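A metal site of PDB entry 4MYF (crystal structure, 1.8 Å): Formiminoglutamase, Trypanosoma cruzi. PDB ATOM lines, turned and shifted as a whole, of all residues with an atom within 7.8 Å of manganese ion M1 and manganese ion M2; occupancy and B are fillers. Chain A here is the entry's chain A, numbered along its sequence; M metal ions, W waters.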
ATOM      1  N   GLY A  42     -16.452 -29.089 -19.677  1.00  0.00           N
ATOM      2  CA  GLY A  42     -15.415 -28.275 -19.052  1.00  0.00           C
ATOM      3  C   GLY A  42     -15.461 -28.488 -17.546  1.00  0.00           C
ATOM      4  O   GLY A  42     -15.343 -29.619 -17.082  1.00  0.00           O
ATOM      5  N   CYS A  43     -15.656 -27.410 -16.795  1.00  0.00           N
ATOM      6  CA  CYS A  43     -15.644 -27.516 -15.333  1.00  0.00           C
ATOM      7  C   CYS A  43     -16.822 -28.303 -14.738  1.00  0.00           C
ATOM      8  O   CYS A  43     -16.782 -28.668 -13.560  1.00  0.00           O
ATOM      9  CB  CYS A  43     -15.544 -26.128 -14.676  1.00  0.00           C
ATOM     10  SG  CYS A  43     -15.036 -26.176 -12.948  1.00  0.00           S
ATOM     11  N   ASN A  46     -15.576 -31.214 -13.151  1.00  0.00           N
ATOM     12  CA  ASN A  46     -14.873 -30.966 -11.897  1.00  0.00           C
ATOM     13  C   ASN A  46     -15.813 -30.469 -10.813  1.00  0.00           C
ATOM     14  O   ASN A  46     -15.505 -29.523 -10.091  1.00  0.00           O
ATOM     15  CB  ASN A  46     -13.739 -29.954 -12.105  1.00  0.00           C
ATOM     16  CG  ASN A  46     -12.726 -30.410 -13.134  1.00  0.00           C
ATOM     17  OD1 ASN A  46     -12.867 -31.476 -13.752  1.00  0.00           O
ATOM     18  ND2 ASN A  46     -11.676 -29.611 -13.321  1.00  0.00           N
ATOM     19  N   GLY A 121     -18.319 -24.848 -22.386  1.00  0.00           N
ATOM     20  CA  GLY A 121     -17.308 -25.212 -21.411  1.00  0.00           C
ATOM     21  C   GLY A 121     -15.851 -25.068 -21.878  1.00  0.00           C
ATOM     22  O   GLY A 121     -15.596 -24.864 -23.079  1.00  0.00           O
ATOM     23  N   ASN A 122     -14.927 -25.176 -20.917  1.00  0.00           N
ATOM     24  CA  ASN A 122     -13.476 -25.069 -21.119  1.00  0.00           C
ATOM     25  C   ASN A 122     -12.917 -25.912 -22.254  1.00  0.00           C
ATOM     26  O   ASN A 122     -11.872 -25.578 -22.832  1.00  0.00           O
ATOM     27  CB  ASN A 122     -12.704 -25.550 -19.884  1.00  0.00           C
ATOM     28  CG  ASN A 122     -12.824 -24.620 -18.703  1.00  0.00           C
ATOM     29  OD1 ASN A 122     -12.649 -23.395 -18.819  1.00  0.00           O
ATOM     30  ND2 ASN A 122     -13.048 -25.209 -17.528  1.00  0.00           N
ATOM     31  N   ASP A 123     -13.562 -27.036 -22.527  1.00  0.00           N
ATOM     32  CA  ASP A 123     -13.009 -27.985 -23.498  1.00  0.00           C
ATOM     33  C   ASP A 123     -12.831 -27.368 -24.884  1.00  0.00           C
ATOM     34  O   ASP A 123     -12.015 -27.830 -25.679  1.00  0.00           O
ATOM     35  CB  ASP A 123     -13.835 -29.274 -23.543  1.00  0.00           C
ATOM     36  CG  ASP A 123     -13.603 -30.162 -22.324  1.00  0.00           C
ATOM     37  OD1 ASP A 123     -12.907 -29.713 -21.388  1.00  0.00           O
ATOM     38  OD2 ASP A 123     -14.102 -31.307 -22.298  1.00  0.00           O
ATOM     39  N   SER A 125     -11.264 -24.844 -25.667  1.00  0.00           N
ATOM     40  CA  SER A 125      -9.967 -24.200 -25.816  1.00  0.00           C
ATOM     41  C   SER A 125      -8.921 -25.120 -26.466  1.00  0.00           C
ATOM     42  O   SER A 125      -7.939 -24.637 -27.010  1.00  0.00           O
ATOM     43  CB  SER A 125      -9.443 -23.711 -24.456  1.00  0.00           C
ATOM     44  OG  SER A 125     -10.394 -22.882 -23.824  1.00  0.00           O
ATOM     45  N   ASN A 144      -4.038 -18.924 -20.166  1.00  0.00           N
ATOM     46  CA  ASN A 144      -5.282 -19.426 -19.621  1.00  0.00           C
ATOM     47  C   ASN A 144      -5.614 -18.634 -18.354  1.00  0.00           C
ATOM     48  O   ASN A 144      -4.963 -18.822 -17.307  1.00  0.00           O
ATOM     49  CB  ASN A 144      -5.191 -20.919 -19.287  1.00  0.00           C
ATOM     50  CG  ASN A 144      -6.471 -21.461 -18.650  1.00  0.00           C
ATOM     51  OD1 ASN A 144      -7.564 -20.961 -18.938  1.00  0.00           O
ATOM     52  ND2 ASN A 144      -6.330 -22.474 -17.808  1.00  0.00           N
ATOM     53  N   VAL A 145      -6.611 -17.762 -18.461  1.00  0.00           N
ATOM     54  CA  VAL A 145      -7.100 -16.989 -17.337  1.00  0.00           C
ATOM     55  C   VAL A 145      -8.157 -17.886 -16.694  1.00  0.00           C
ATOM     56  O   VAL A 145      -9.200 -18.127 -17.304  1.00  0.00           O
ATOM     57  CB  VAL A 145      -7.732 -15.651 -17.782  1.00  0.00           C
ATOM     58  CG1 VAL A 145      -8.325 -14.902 -16.577  1.00  0.00           C
ATOM     59  CG2 VAL A 145      -6.715 -14.765 -18.506  1.00  0.00           C
ATOM     60  N   ASP A 146      -7.858 -18.399 -15.512  1.00  0.00           N
ATOM     61  CA  ASP A 146      -8.662 -19.456 -14.931  1.00  0.00           C
ATOM     62  C   ASP A 146      -8.330 -19.620 -13.448  1.00  0.00           C
ATOM     63  O   ASP A 146      -7.164 -19.598 -13.061  1.00  0.00           O
ATOM     64  CB  ASP A 146      -8.361 -20.762 -15.667  1.00  0.00           C
ATOM     65  CG  ASP A 146      -9.393 -21.852 -15.411  1.00  0.00           C
ATOM     66  OD1 ASP A 146     -10.210 -21.725 -14.474  1.00  0.00           O
ATOM     67  OD2 ASP A 146      -9.357 -22.847 -16.158  1.00  0.00           O
ATOM     68  N   SER A 147      -9.357 -19.760 -12.613  1.00  0.00           N
ATOM     69  CA  SER A 147      -9.082 -20.043 -11.201  1.00  0.00           C
ATOM     70  C   SER A 147      -8.499 -21.456 -11.065  1.00  0.00           C
ATOM     71  O   SER A 147      -7.818 -21.748 -10.100  1.00  0.00           O
ATOM     72  CB  SER A 147     -10.324 -19.866 -10.337  1.00  0.00           C
ATOM     73  OG  SER A 147     -11.351 -20.751 -10.733  1.00  0.00           O
ATOM     74  N   HIS A 148      -8.749 -22.314 -12.068  1.00  0.00           N
ATOM     75  CA  HIS A 148      -8.272 -23.711 -12.089  1.00  0.00           C
ATOM     76  C   HIS A 148      -7.139 -23.902 -13.115  1.00  0.00           C
ATOM     77  O   HIS A 148      -7.023 -23.124 -14.053  1.00  0.00           O
ATOM     78  CB  HIS A 148      -9.425 -24.648 -12.464  1.00  0.00           C
ATOM     79  CG  HIS A 148     -10.718 -24.372 -11.754  1.00  0.00           C
ATOM     80  ND1 HIS A 148     -11.689 -23.542 -12.252  1.00  0.00           N
ATOM     81  CD2 HIS A 148     -11.193 -24.846 -10.571  1.00  0.00           C
ATOM     82  CE1 HIS A 148     -12.708 -23.485 -11.417  1.00  0.00           C
ATOM     83  NE2 HIS A 148     -12.435 -24.279 -10.389  1.00  0.00           N
ATOM     84  N   LEU A 149      -6.312 -24.949 -12.968  1.00  0.00           N
ATOM     85  CA  LEU A 149      -5.233 -25.179 -13.958  1.00  0.00           C
ATOM     86  C   LEU A 149      -5.642 -25.815 -15.302  1.00  0.00           C
ATOM     87  O   LEU A 149      -4.972 -25.609 -16.336  1.00  0.00           O
ATOM     88  CB  LEU A 149      -4.073 -25.976 -13.341  1.00  0.00           C
ATOM     89  CG  LEU A 149      -3.098 -25.248 -12.419  1.00  0.00           C
ATOM     90  CD1 LEU A 149      -1.901 -26.143 -12.206  1.00  0.00           C
ATOM     91  CD2 LEU A 149      -2.652 -23.924 -13.005  1.00  0.00           C
ATOM     92  N   ASP A 150      -6.716 -26.594 -15.276  1.00  0.00           N
ATOM     93  CA  ASP A 150      -7.216 -27.290 -16.481  1.00  0.00           C
ATOM     94  C   ASP A 150      -6.162 -28.182 -17.140  1.00  0.00           C
ATOM     95  O   ASP A 150      -5.939 -28.093 -18.357  1.00  0.00           O
ATOM     96  CB  ASP A 150      -7.733 -26.278 -17.511  1.00  0.00           C
ATOM     97  CG  ASP A 150      -9.126 -25.781 -17.216  1.00  0.00           C
ATOM     98  OD1 ASP A 150      -9.594 -25.921 -16.057  1.00  0.00           O
ATOM     99  OD2 ASP A 150      -9.754 -25.222 -18.150  1.00  0.00           O
ATOM    100  N   PRO A 165      -8.208 -29.212 -21.628  1.00  0.00           N
ATOM    101  CA  PRO A 165      -7.770 -28.553 -22.858  1.00  0.00           C
ATOM    102  C   PRO A 165      -6.299 -28.111 -22.847  1.00  0.00           C
ATOM    103  O   PRO A 165      -5.648 -28.155 -23.899  1.00  0.00           O
ATOM    104  CB  PRO A 165      -8.701 -27.335 -22.948  1.00  0.00           C
ATOM    105  CG  PRO A 165      -9.184 -27.097 -21.531  1.00  0.00           C
ATOM    106  CD  PRO A 165      -9.299 -28.490 -20.957  1.00  0.00           C
ATOM    107  N   PHE A 166      -5.760 -27.709 -21.700  1.00  0.00           N
ATOM    108  CA  PHE A 166      -4.373 -27.244 -21.704  1.00  0.00           C
ATOM    109  C   PHE A 166      -3.329 -28.330 -21.488  1.00  0.00           C
ATOM    110  O   PHE A 166      -2.144 -28.139 -21.767  1.00  0.00           O
ATOM    111  CB  PHE A 166      -4.197 -26.021 -20.783  1.00  0.00           C
ATOM    112  CG  PHE A 166      -5.105 -24.901 -21.177  1.00  0.00           C
ATOM    113  CD1 PHE A 166      -4.801 -24.100 -22.265  1.00  0.00           C
ATOM    114  CD2 PHE A 166      -6.304 -24.702 -20.525  1.00  0.00           C
ATOM    115  CE1 PHE A 166      -5.660 -23.090 -22.678  1.00  0.00           C
ATOM    116  CE2 PHE A 166      -7.168 -23.685 -20.933  1.00  0.00           C
ATOM    117  CZ  PHE A 166      -6.841 -22.872 -21.995  1.00  0.00           C
ATOM    118  N   GLU A 182      -0.537 -19.692 -16.888  1.00  0.00           N
ATOM    119  CA  GLU A 182      -1.746 -19.905 -16.114  1.00  0.00           C
ATOM    120  C   GLU A 182      -1.915 -18.645 -15.269  1.00  0.00           C
ATOM    121  O   GLU A 182      -1.077 -18.345 -14.422  1.00  0.00           O
ATOM    122  CB  GLU A 182      -1.597 -21.134 -15.215  1.00  0.00           C
ATOM    123  CG  GLU A 182      -1.360 -22.448 -15.965  1.00  0.00           C
ATOM    124  CD  GLU A 182      -2.650 -23.168 -16.331  1.00  0.00           C
ATOM    125  OE1 GLU A 182      -3.719 -22.519 -16.450  1.00  0.00           O
ATOM    126  OE2 GLU A 182      -2.594 -24.408 -16.504  1.00  0.00           O
ATOM    127  N   GLN A 189      -7.288 -24.479  -5.141  1.00  0.00           N
ATOM    128  CA  GLN A 189      -7.935 -25.238  -6.218  1.00  0.00           C
ATOM    129  C   GLN A 189      -6.963 -25.866  -7.199  1.00  0.00           C
ATOM    130  O   GLN A 189      -7.367 -26.227  -8.305  1.00  0.00           O
ATOM    131  CB  GLN A 189      -8.803 -24.300  -7.056  1.00  0.00           C
ATOM    132  CG  GLN A 189      -9.990 -23.719  -6.352  1.00  0.00           C
ATOM    133  CD  GLN A 189     -11.065 -23.399  -7.351  1.00  0.00           C
ATOM    134  OE1 GLN A 189     -12.213 -23.808  -7.190  1.00  0.00           O
ATOM    135  NE2 GLN A 189     -10.683 -22.690  -8.417  1.00  0.00           N
ATOM    136  N   SER A 234      -7.216 -16.809 -23.556  1.00  0.00           N
ATOM    137  CA  SER A 234      -8.297 -17.751 -23.198  1.00  0.00           C
ATOM    138  C   SER A 234      -8.845 -17.401 -21.817  1.00  0.00           C
ATOM    139  O   SER A 234      -8.140 -17.533 -20.808  1.00  0.00           O
ATOM    140  CB  SER A 234      -7.762 -19.186 -23.208  1.00  0.00           C
ATOM    141  OG  SER A 234      -8.804 -20.146 -23.109  1.00  0.00           O
ATOM    142  N   PHE A 235     -10.102 -16.968 -21.761  1.00  0.00           N
ATOM    143  CA  PHE A 235     -10.643 -16.380 -20.547  1.00  0.00           C
ATOM    144  C   PHE A 235     -11.772 -17.238 -19.983  1.00  0.00           C
ATOM    145  O   PHE A 235     -12.900 -17.150 -20.455  1.00  0.00           O
ATOM    146  CB  PHE A 235     -11.163 -14.958 -20.824  1.00  0.00           C
ATOM    147  CG  PHE A 235     -11.049 -14.023 -19.634  1.00  0.00           C
ATOM    148  CD1 PHE A 235     -11.423 -14.450 -18.374  1.00  0.00           C
ATOM    149  CD2 PHE A 235     -10.568 -12.722 -19.800  1.00  0.00           C
ATOM    150  CE1 PHE A 235     -11.317 -13.594 -17.278  1.00  0.00           C
ATOM    151  CE2 PHE A 235     -10.476 -11.864 -18.700  1.00  0.00           C
ATOM    152  CZ  PHE A 235     -10.844 -12.298 -17.446  1.00  0.00           C
ATOM    153  N   ASP A 236     -11.457 -18.070 -19.000  1.00  0.00           N
ATOM    154  CA  ASP A 236     -12.462 -18.827 -18.260  1.00  0.00           C
ATOM    155  C   ASP A 236     -13.079 -17.885 -17.230  1.00  0.00           C
ATOM    156  O   ASP A 236     -12.390 -17.438 -16.317  1.00  0.00           O
ATOM    157  CB  ASP A 236     -11.804 -20.038 -17.576  1.00  0.00           C
ATOM    158  CG  ASP A 236     -12.773 -20.888 -16.758  1.00  0.00           C
ATOM    159  OD1 ASP A 236     -13.885 -20.447 -16.444  1.00  0.00           O
ATOM    160  OD2 ASP A 236     -12.404 -22.016 -16.398  1.00  0.00           O
ATOM    161  N   VAL A 237     -14.365 -17.561 -17.401  1.00  0.00           N
ATOM    162  CA  VAL A 237     -14.990 -16.544 -16.550  1.00  0.00           C
ATOM    163  C   VAL A 237     -15.209 -16.981 -15.093  1.00  0.00           C
ATOM    164  O   VAL A 237     -15.591 -16.158 -14.251  1.00  0.00           O
ATOM    165  CB  VAL A 237     -16.316 -15.958 -17.149  1.00  0.00           C
ATOM    166  CG1 VAL A 237     -16.013 -15.153 -18.413  1.00  0.00           C
ATOM    167  CG2 VAL A 237     -17.333 -17.059 -17.429  1.00  0.00           C
ATOM    168  N   ASP A 238     -14.975 -18.260 -14.782  1.00  0.00           N
ATOM    169  CA  ASP A 238     -15.003 -18.648 -13.375  1.00  0.00           C
ATOM    170  C   ASP A 238     -13.719 -18.206 -12.677  1.00  0.00           C
ATOM    171  O   ASP A 238     -13.480 -18.542 -11.516  1.00  0.00           O
ATOM    172  CB  ASP A 238     -15.325 -20.147 -13.200  1.00  0.00           C
ATOM    173  CG  ASP A 238     -14.177 -21.065 -13.587  1.00  0.00           C
ATOM    174  OD1 ASP A 238     -12.995 -20.639 -13.567  1.00  0.00           O
ATOM    175  OD2 ASP A 238     -14.472 -22.248 -13.882  1.00  0.00           O
ATOM    176  N   SER A 239     -12.896 -17.432 -13.387  1.00  0.00           N
ATOM    177  CA  SER A 239     -11.757 -16.782 -12.755  1.00  0.00           C
ATOM    178  C   SER A 239     -12.213 -15.511 -12.027  1.00  0.00           C
ATOM    179  O   SER A 239     -11.465 -14.942 -11.233  1.00  0.00           O
ATOM    180  CB  SER A 239     -10.673 -16.422 -13.779  1.00  0.00           C
ATOM    181  OG  SER A 239     -11.160 -15.510 -14.746  1.00  0.00           O
ATOM    182  N   VAL A 248     -21.649 -19.165 -13.503  1.00  0.00           N
ATOM    183  CA  VAL A 248     -20.619 -19.993 -14.117  1.00  0.00           C
ATOM    184  C   VAL A 248     -20.776 -21.395 -13.551  1.00  0.00           C
ATOM    185  O   VAL A 248     -21.405 -21.592 -12.509  1.00  0.00           O
ATOM    186  CB  VAL A 248     -19.186 -19.479 -13.839  1.00  0.00           C
ATOM    187  CG1 VAL A 248     -19.025 -18.056 -14.370  1.00  0.00           C
ATOM    188  CG2 VAL A 248     -18.860 -19.578 -12.350  1.00  0.00           C
ATOM    189  N   CYS A 250     -18.652 -23.369 -12.133  1.00  0.00           N
ATOM    190  CA  CYS A 250     -17.907 -23.526 -10.886  1.00  0.00           C
ATOM    191  C   CYS A 250     -17.621 -22.166 -10.242  1.00  0.00           C
ATOM    192  O   CYS A 250     -16.540 -21.612 -10.406  1.00  0.00           O
ATOM    193  CB  CYS A 250     -16.572 -24.216 -11.177  1.00  0.00           C
ATOM    194  SG  CYS A 250     -16.760 -25.861 -11.911  1.00  0.00           S
ATOM    195  N   SER A 280     -14.950 -18.982 -21.728  1.00  0.00           N
ATOM    196  CA  SER A 280     -15.547 -20.259 -21.365  1.00  0.00           C
ATOM    197  C   SER A 280     -16.267 -20.191 -20.033  1.00  0.00           C
ATOM    198  O   SER A 280     -15.976 -19.337 -19.209  1.00  0.00           O
ATOM    199  CB  SER A 280     -14.469 -21.349 -21.279  1.00  0.00           C
ATOM    200  OG  SER A 280     -13.849 -21.559 -22.544  1.00  0.00           O
ATOM    201  N   GLU A 281     -17.199 -21.122 -19.846  1.00  0.00           N
ATOM    202  CA  GLU A 281     -17.866 -21.426 -18.574  1.00  0.00           C
ATOM    203  C   GLU A 281     -19.058 -20.552 -18.192  1.00  0.00           C
ATOM    204  O   GLU A 281     -19.605 -20.703 -17.093  1.00  0.00           O
ATOM    205  CB  GLU A 281     -16.849 -21.540 -17.423  1.00  0.00           C
ATOM    206  CG  GLU A 281     -15.805 -22.662 -17.611  1.00  0.00           C
ATOM    207  CD  GLU A 281     -16.423 -24.049 -17.597  1.00  0.00           C
ATOM    208  OE1 GLU A 281     -17.420 -24.248 -16.865  1.00  0.00           O
ATOM    209  OE2 GLU A 281     -15.903 -24.955 -18.296  1.00  0.00           O
HETATM  210 MN    MN M   1     -12.183 -22.666 -14.289  1.00  0.00          MN
HETATM  211 MN    MN M   2     -11.143 -23.627 -17.090  1.00  0.00          MN
HETATM  212  O   HOH W   1     -11.723 -24.708 -15.214  1.00  0.00           O
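N of Asp 236 is in hydrogen-bond range of O of Val 145 (2.8 Å).
The side-chain amide nitrogen (ND2) of Asn 144 lies close to the side-chain carboxylate (OD2) of Asp 146 (3.5 Å).
A ring nitrogen (NE2) of His 148 sits at hydrogen-bond distance from the side-chain amide nitrogen (NE2) of Gln 189 (3.1 Å).
The side-chain hydroxyl of Ser 147 is in hydrogen-bond range of the backbone carbonyl oxygen of Asp 238, at 3.2 Å.
The side-chain amide nitrogen (ND2) of Asn 122 sits close to the backbone NH (N) of Cys 43 (3.5 Å).
O of Asn 122 lies within hydrogen-bond range of OG of Ser 125, 3.2 Å away.
The backbone NH (N) of Phe 166 lies within hydrogen-bond range of the backbone carbonyl oxygen (O) of Asp 150, at 3.4 Å.
The side-chain sulfur of Cys 43 is disulfide-bonded to the side-chain sulfur of Cys 250.
Four residues have an atom within 4 Å of manganese ion M1: Asp 146, His 148, Asp 236 and Asp 238.
Of the 28 residues printed, 4 come within 4 Å of manganese ion M2.
Manganese ion M1 is bound by the side-chain carboxylate (OD1) of Asp 146, the side-chain carboxylate (OD2) of Asp 236, a ring nitrogen (ND1) of His 148, water W1, the side-chain carboxylate (OD1) of Asp 238 and the side-chain carboxylate (OD2) of Asp 238.
OD2 of Asp 236 is bound to manganese ion M2 (2.2 Å).
Manganese ion M2 is bound by the side-chain carboxylate (OD2) of Asp 146, at 2.2 Å.
Water W1 is bound to manganese ion M2, at 2.2 Å.
Manganese ion M2 is bound by OD1 of Asn 122 (2.3 Å).
The side-chain carboxylate (OD2) of Asp 150 binds manganese ion M2, at 2.4 Å.
ND2 of Asn 122 is bound to manganese ion M2 (2.5 Å).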
